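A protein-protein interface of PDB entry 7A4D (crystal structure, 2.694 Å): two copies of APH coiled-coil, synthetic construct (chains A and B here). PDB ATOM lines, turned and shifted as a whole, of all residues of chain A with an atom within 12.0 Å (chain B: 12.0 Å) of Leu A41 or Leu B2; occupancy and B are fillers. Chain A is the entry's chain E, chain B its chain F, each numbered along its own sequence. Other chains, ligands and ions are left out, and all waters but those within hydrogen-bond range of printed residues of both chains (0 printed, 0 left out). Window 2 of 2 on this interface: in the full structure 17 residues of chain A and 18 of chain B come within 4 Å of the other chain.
No position is printed for both chains.
Of the 6 pairs that touch across the chains among the printed residues, none has its exchanged pair printed and touching as well.
Leu B6 touches Leu A34.
Leu A34 touches Leu B9.
Leu A34 touches Glu B10.
Leu A37 touches Glu B5 (CD1 to CG, 3.8 Å).
Leu A41 touches Leu B2 (CD2 to CB, 3.9 Å).
Of chain A, only Leu A41 (3.9 Å) comes within 4 Å of Leu B2.
Leu A37 touches one residue of chain B.
No residue of chain B comes within 4 Å of NH2 A42.
No residue of chain A comes within 4 Å of ACE B1.
No residue of chain A comes within 4 Å of Glu B3.
Of chain A, only Leu A37 comes within 4 Å of Glu B5.
Of chain A, only Leu A34 (3.2 Å) comes within 4 Å of Leu B6.
Of the printed residues of chain A, Leu B9 touches Leu A34 (3.8 Å).
Of the printed residues of chain B, Lys A38 touches Glu B10 (3.5 Å).
Of the printed residues of chain B, Leu A34 touches Leu B6, Leu B9 and Glu B10.
Lys A33 touches none of the printed residues of chain B.
Gln B8 touches none of the printed residues of chain A.
The nearest residue of chain B that does not touch Leu A41 is Leu B6 (4.2 Å).
OE2 of Glu B10 lies within salt-bridge range of NZ of Lys A38.
Of the 11 printed residues of chain B, 5 touch a printed residue of chain A.
Along chain B the printed residues that touch a printed residue of chain A span positions 2 to 10.
Of the 11 printed residues of chain A, 4 touch a printed residue of chain B.
Hydrophobic or aromatic side chains of chain A within 4 Å of the printed part of chain B: Leu A34, Leu A37 and Leu A41.
Among the printed residues, 6 pairs touch across the chains.
Among the printed residues, Asp or Glu carboxylates within 4 Å of a Lys or Arg side-chain nitrogen of the other chain: Lys A38 with Glu B10 (3.5 Å).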
ATOM      1  N   GLU A  32     -20.306  -1.549  16.909  1.00  0.00           N
ATOM      2  CA  GLU A  32     -19.603  -0.287  17.077  1.00  0.00           C
ATOM      3  C   GLU A  32     -18.221  -0.325  16.427  1.00  0.00           C
ATOM      4  O   GLU A  32     -17.812   0.632  15.769  1.00  0.00           O
ATOM      5  CB  GLU A  32     -19.502   0.048  18.560  1.00  0.00           C
ATOM      6  CG  GLU A  32     -20.774   0.601  19.140  1.00  0.00           C
ATOM      7  CD  GLU A  32     -20.699   0.817  20.650  1.00  0.00           C
ATOM      8  OE1 GLU A  32     -19.653   1.320  21.134  1.00  0.00           O
ATOM      9  OE2 GLU A  32     -21.707   0.541  21.343  1.00  0.00           O
ATOM     10  N   LYS A  33     -17.479  -1.413  16.609  1.00  0.00           N
ATOM     11  CA  LYS A  33     -16.153  -1.487  16.008  1.00  0.00           C
ATOM     12  C   LYS A  33     -16.249  -1.364  14.501  1.00  0.00           C
ATOM     13  O   LYS A  33     -15.399  -0.729  13.860  1.00  0.00           O
ATOM     14  CB  LYS A  33     -15.448  -2.785  16.414  1.00  0.00           C
ATOM     15  CG  LYS A  33     -13.964  -2.878  16.007  1.00  0.00           C
ATOM     16  CD  LYS A  33     -13.075  -1.911  16.781  1.00  0.00           C
ATOM     17  CE  LYS A  33     -11.608  -1.999  16.317  1.00  0.00           C
ATOM     18  NZ  LYS A  33     -10.746  -0.891  16.901  1.00  0.00           N
ATOM     19  N   LEU A  34     -17.296  -1.956  13.925  1.00  0.00           N
ATOM     20  CA  LEU A  34     -17.513  -1.903  12.483  1.00  0.00           C
ATOM     21  C   LEU A  34     -17.795  -0.475  12.022  1.00  0.00           C
ATOM     22  O   LEU A  34     -17.252  -0.022  11.006  1.00  0.00           O
ATOM     23  CB  LEU A  34     -18.644  -2.864  12.127  1.00  0.00           C
ATOM     24  CG  LEU A  34     -19.117  -3.116  10.702  1.00  0.00           C
ATOM     25  CD1 LEU A  34     -17.931  -3.386   9.822  1.00  0.00           C
ATOM     26  CD2 LEU A  34     -20.049  -4.332  10.704  1.00  0.00           C
ATOM     27  N   ALA A  35     -18.605   0.268  12.779  1.00  0.00           N
ATOM     28  CA  ALA A  35     -18.829   1.667  12.429  1.00  0.00           C
ATOM     29  C   ALA A  35     -17.531   2.462  12.449  1.00  0.00           C
ATOM     30  O   ALA A  35     -17.278   3.262  11.539  1.00  0.00           O
ATOM     31  CB  ALA A  35     -19.836   2.293  13.379  1.00  0.00           C
ATOM     32  N   GLN A  36     -16.695   2.267  13.479  1.00  0.00           N
ATOM     33  CA  GLN A  36     -15.455   3.033  13.547  1.00  0.00           C
ATOM     34  C   GLN A  36     -14.565   2.717  12.361  1.00  0.00           C
ATOM     35  O   GLN A  36     -13.916   3.610  11.808  1.00  0.00           O
ATOM     36  CB  GLN A  36     -14.707   2.780  14.851  1.00  0.00           C
ATOM     37  CG  GLN A  36     -15.508   3.075  16.100  1.00  0.00           C
ATOM     38  CD  GLN A  36     -14.928   2.388  17.340  1.00  0.00           C
ATOM     39  OE1 GLN A  36     -13.784   1.901  17.332  1.00  0.00           O
ATOM     40  NE2 GLN A  36     -15.727   2.325  18.404  1.00  0.00           N
ATOM     41  N   LEU A  37     -14.515   1.451  11.950  1.00  0.00           N
ATOM     42  CA  LEU A  37     -13.728   1.121  10.768  1.00  0.00           C
ATOM     43  C   LEU A  37     -14.292   1.827   9.545  1.00  0.00           C
ATOM     44  O   LEU A  37     -13.550   2.449   8.772  1.00  0.00           O
ATOM     45  CB  LEU A  37     -13.730  -0.387  10.535  1.00  0.00           C
ATOM     46  CG  LEU A  37     -12.605  -1.187  11.158  1.00  0.00           C
ATOM     47  CD1 LEU A  37     -12.689  -2.586  10.620  1.00  0.00           C
ATOM     48  CD2 LEU A  37     -11.242  -0.542  10.890  1.00  0.00           C
ATOM     49  N   LYS A  38     -15.619   1.801   9.394  1.00  0.00           N
ATOM     50  CA  LYS A  38     -16.230   2.466   8.252  1.00  0.00           C
ATOM     51  C   LYS A  38     -15.849   3.945   8.214  1.00  0.00           C
ATOM     52  O   LYS A  38     -15.479   4.465   7.154  1.00  0.00           O
ATOM     53  CB  LYS A  38     -17.742   2.263   8.287  1.00  0.00           C
ATOM     54  CG  LYS A  38     -18.196   1.109   7.385  1.00  0.00           C
ATOM     55  CD  LYS A  38     -19.568   0.594   7.749  1.00  0.00           C
ATOM     56  CE  LYS A  38     -20.063  -0.447   6.721  1.00  0.00           C
ATOM     57  NZ  LYS A  38     -21.162  -1.311   7.291  1.00  0.00           N
ATOM     58  N   GLU A  39     -15.855   4.623   9.371  1.00  0.00           N
ATOM     59  CA  GLU A  39     -15.465   6.033   9.363  1.00  0.00           C
ATOM     60  C   GLU A  39     -13.995   6.219   9.028  1.00  0.00           C
ATOM     61  O   GLU A  39     -13.640   7.228   8.419  1.00  0.00           O
ATOM     62  CB  GLU A  39     -15.701   6.695  10.725  1.00  0.00           C
ATOM     63  CG  GLU A  39     -17.010   7.464  10.916  1.00  0.00           C
ATOM     64  CD  GLU A  39     -16.979   8.371  12.165  1.00  0.00           C
ATOM     65  OE1 GLU A  39     -15.872   8.719  12.638  1.00  0.00           O
ATOM     66  OE2 GLU A  39     -18.066   8.731  12.676  1.00  0.00           O
ATOM     67  N   LYS A  40     -13.134   5.253   9.367  1.00  0.00           N
ATOM     68  CA  LYS A  40     -11.719   5.401   9.039  1.00  0.00           C
ATOM     69  C   LYS A  40     -11.463   5.346   7.543  1.00  0.00           C
ATOM     70  O   LYS A  40     -10.402   5.787   7.092  1.00  0.00           O
ATOM     71  CB  LYS A  40     -10.870   4.359   9.767  1.00  0.00           C
ATOM     72  CG  LYS A  40     -10.763   4.596  11.265  1.00  0.00           C
ATOM     73  CD  LYS A  40      -9.826   3.580  11.949  1.00  0.00           C
ATOM     74  CE  LYS A  40      -9.887   3.705  13.487  1.00  0.00           C
ATOM     75  NZ  LYS A  40      -9.106   2.635  14.184  1.00  0.00           N
ATOM     76  N   LEU A  41     -12.381   4.764   6.779  1.00  0.00           N
ATOM     77  CA  LEU A  41     -12.324   4.805   5.321  1.00  0.00           C
ATOM     78  C   LEU A  41     -12.611   6.200   4.756  1.00  0.00           C
ATOM     79  O   LEU A  41     -12.229   6.498   3.615  1.00  0.00           O
ATOM     80  CB  LEU A  41     -13.307   3.788   4.733  1.00  0.00           C
ATOM     81  CG  LEU A  41     -13.097   2.299   5.076  1.00  0.00           C
ATOM     82  CD1 LEU A  41     -14.021   1.460   4.253  1.00  0.00           C
ATOM     83  CD2 LEU A  41     -11.659   1.858   4.871  1.00  0.00           C
ATOM     84  N   NH2 A  42     -13.272   7.049   5.546  1.00  0.00           N
ATOM     85  C   ACE B   1      -6.927  -3.723   5.427  1.00  0.00           C
ATOM     86  O   ACE B   1      -7.559  -4.554   6.075  1.00  0.00           O
ATOM     87  CH3 ACE B   1      -5.643  -4.119   4.691  1.00  0.00           C
ATOM     88  N   LEU B   2      -7.288  -2.439   5.318  1.00  0.00           N
ATOM     89  CA  LEU B   2      -8.513  -1.932   5.932  1.00  0.00           C
ATOM     90  C   LEU B   2      -9.747  -2.646   5.385  1.00  0.00           C
ATOM     91  O   LEU B   2     -10.612  -3.080   6.156  1.00  0.00           O
ATOM     92  CB  LEU B   2      -8.622  -0.423   5.734  1.00  0.00           C
ATOM     93  N   GLU B   3      -9.869  -2.742   4.052  1.00  0.00           N
ATOM     94  CA  GLU B   3     -11.008  -3.450   3.455  1.00  0.00           C
ATOM     95  C   GLU B   3     -11.104  -4.898   3.940  1.00  0.00           C
ATOM     96  O   GLU B   3     -12.201  -5.392   4.236  1.00  0.00           O
ATOM     97  CB  GLU B   3     -10.913  -3.399   1.929  1.00  0.00           C
ATOM     98  N   GLU B   4      -9.976  -5.606   4.004  1.00  0.00           N
ATOM     99  CA  GLU B   4      -9.998  -6.993   4.467  1.00  0.00           C
ATOM    100  C   GLU B   4     -10.542  -7.090   5.892  1.00  0.00           C
ATOM    101  O   GLU B   4     -11.405  -7.926   6.188  1.00  0.00           O
ATOM    102  CB  GLU B   4      -8.590  -7.588   4.373  1.00  0.00           C
ATOM    103  CG  GLU B   4      -8.516  -9.088   4.641  1.00  0.00           C
ATOM    104  CD  GLU B   4      -7.147  -9.676   4.334  1.00  0.00           C
ATOM    105  OE1 GLU B   4      -6.652  -9.520   3.193  1.00  0.00           O
ATOM    106  OE2 GLU B   4      -6.565 -10.297   5.248  1.00  0.00           O
ATOM    107  N   GLU B   5     -10.024  -6.256   6.797  1.00  0.00           N
ATOM    108  CA  GLU B   5     -10.520  -6.248   8.168  1.00  0.00           C
ATOM    109  C   GLU B   5     -12.022  -6.004   8.207  1.00  0.00           C
ATOM    110  O   GLU B   5     -12.726  -6.563   9.059  1.00  0.00           O
ATOM    111  CB  GLU B   5      -9.772  -5.183   8.974  1.00  0.00           C
ATOM    112  CG  GLU B   5     -10.013  -5.216  10.468  1.00  0.00           C
ATOM    113  CD  GLU B   5      -8.993  -4.377  11.244  1.00  0.00           C
ATOM    114  OE1 GLU B   5      -8.075  -3.798  10.615  1.00  0.00           O
ATOM    115  OE2 GLU B   5      -9.093  -4.319  12.490  1.00  0.00           O
ATOM    116  N   LEU B   6     -12.531  -5.221   7.250  1.00  0.00           N
ATOM    117  CA  LEU B   6     -13.938  -4.839   7.243  1.00  0.00           C
ATOM    118  C   LEU B   6     -14.845  -6.028   6.920  1.00  0.00           C
ATOM    119  O   LEU B   6     -15.830  -6.276   7.620  1.00  0.00           O
ATOM    120  CB  LEU B   6     -14.155  -3.694   6.255  1.00  0.00           C
ATOM    121  CG  LEU B   6     -15.572  -3.148   6.370  1.00  0.00           C
ATOM    122  CD1 LEU B   6     -15.688  -2.470   7.700  1.00  0.00           C
ATOM    123  CD2 LEU B   6     -15.900  -2.184   5.236  1.00  0.00           C
ATOM    124  N   LYS B   7     -14.547  -6.767   5.850  1.00  0.00           N
ATOM    125  CA  LYS B   7     -15.373  -7.930   5.552  1.00  0.00           C
ATOM    126  C   LYS B   7     -15.350  -8.921   6.711  1.00  0.00           C
ATOM    127  O   LYS B   7     -16.371  -9.559   6.998  1.00  0.00           O
ATOM    128  CB  LYS B   7     -14.905  -8.599   4.261  1.00  0.00           C
ATOM    129  CG  LYS B   7     -15.997  -8.808   3.202  1.00  0.00           C
ATOM    130  CD  LYS B   7     -17.027  -9.886   3.595  1.00  0.00           C
ATOM    131  CE  LYS B   7     -18.088 -10.123   2.503  1.00  0.00           C
ATOM    132  NZ  LYS B   7     -19.057 -11.211   2.865  1.00  0.00           N
ATOM    133  N   GLN B   8     -14.219  -9.033   7.415  1.00  0.00           N
ATOM    134  CA  GLN B   8     -14.149  -9.940   8.557  1.00  0.00           C
ATOM    135  C   GLN B   8     -15.078  -9.494   9.687  1.00  0.00           C
ATOM    136  O   GLN B   8     -15.762 -10.323  10.302  1.00  0.00           O
ATOM    137  CB  GLN B   8     -12.706 -10.042   9.040  1.00  0.00           C
ATOM    138  CG  GLN B   8     -11.803 -10.639   7.993  1.00  0.00           C
ATOM    139  CD  GLN B   8     -10.337 -10.477   8.315  1.00  0.00           C
ATOM    140  OE1 GLN B   8      -9.966  -9.680   9.173  1.00  0.00           O
ATOM    141  NE2 GLN B   8      -9.487 -11.243   7.628  1.00  0.00           N
ATOM    142  N   LEU B   9     -15.134  -8.188   9.966  1.00  0.00           N
ATOM    143  CA  LEU B   9     -16.050  -7.709  11.000  1.00  0.00           C
ATOM    144  C   LEU B   9     -17.499  -7.995  10.623  1.00  0.00           C
ATOM    145  O   LEU B   9     -18.271  -8.523  11.432  1.00  0.00           O
ATOM    146  CB  LEU B   9     -15.848  -6.212  11.226  1.00  0.00           C
ATOM    147  CG  LEU B   9     -14.827  -5.872  12.302  1.00  0.00           C
ATOM    148  CD1 LEU B   9     -15.329  -6.450  13.628  1.00  0.00           C
ATOM    149  CD2 LEU B   9     -13.447  -6.422  11.925  1.00  0.00           C
ATOM    150  N   GLU B  10     -17.885  -7.641   9.396  1.00  0.00           N
ATOM    151  CA  GLU B  10     -19.241  -7.892   8.924  1.00  0.00           C
ATOM    152  C   GLU B  10     -19.575  -9.373   8.953  1.00  0.00           C
ATOM    153  O   GLU B  10     -20.583  -9.784   9.534  1.00  0.00           O
ATOM    154  CB  GLU B  10     -19.404  -7.341   7.507  1.00  0.00           C
ATOM    155  CG  GLU B  10     -19.578  -5.853   7.466  1.00  0.00           C
ATOM    156  CD  GLU B  10     -19.413  -5.292   6.083  1.00  0.00           C
ATOM    157  OE1 GLU B  10     -18.630  -5.872   5.299  1.00  0.00           O
ATOM    158  OE2 GLU B  10     -20.057  -4.258   5.788  1.00  0.00           O
ATOM    159  N   GLU B  11     -18.730 -10.202   8.348  1.00  0.00           N
ATOM    160  CA  GLU B  11     -19.055 -11.623   8.309  1.00  0.00           C
ATOM    161  C   GLU B  11     -19.188 -12.190   9.720  1.00  0.00           C
ATOM    162  O   GLU B  11     -20.096 -12.984   9.987  1.00  0.00           O
ATOM    163  CB  GLU B  11     -18.013 -12.392   7.491  1.00  0.00           C
ATOM    164  CG  GLU B  11     -18.622 -13.473   6.623  1.00  0.00           C
ATOM    165  CD  GLU B  11     -17.616 -14.543   6.236  1.00  0.00           C
ATOM    166  OE1 GLU B  11     -16.652 -14.189   5.519  1.00  0.00           O
ATOM    167  OE2 GLU B  11     -17.775 -15.723   6.660  1.00  0.00           O
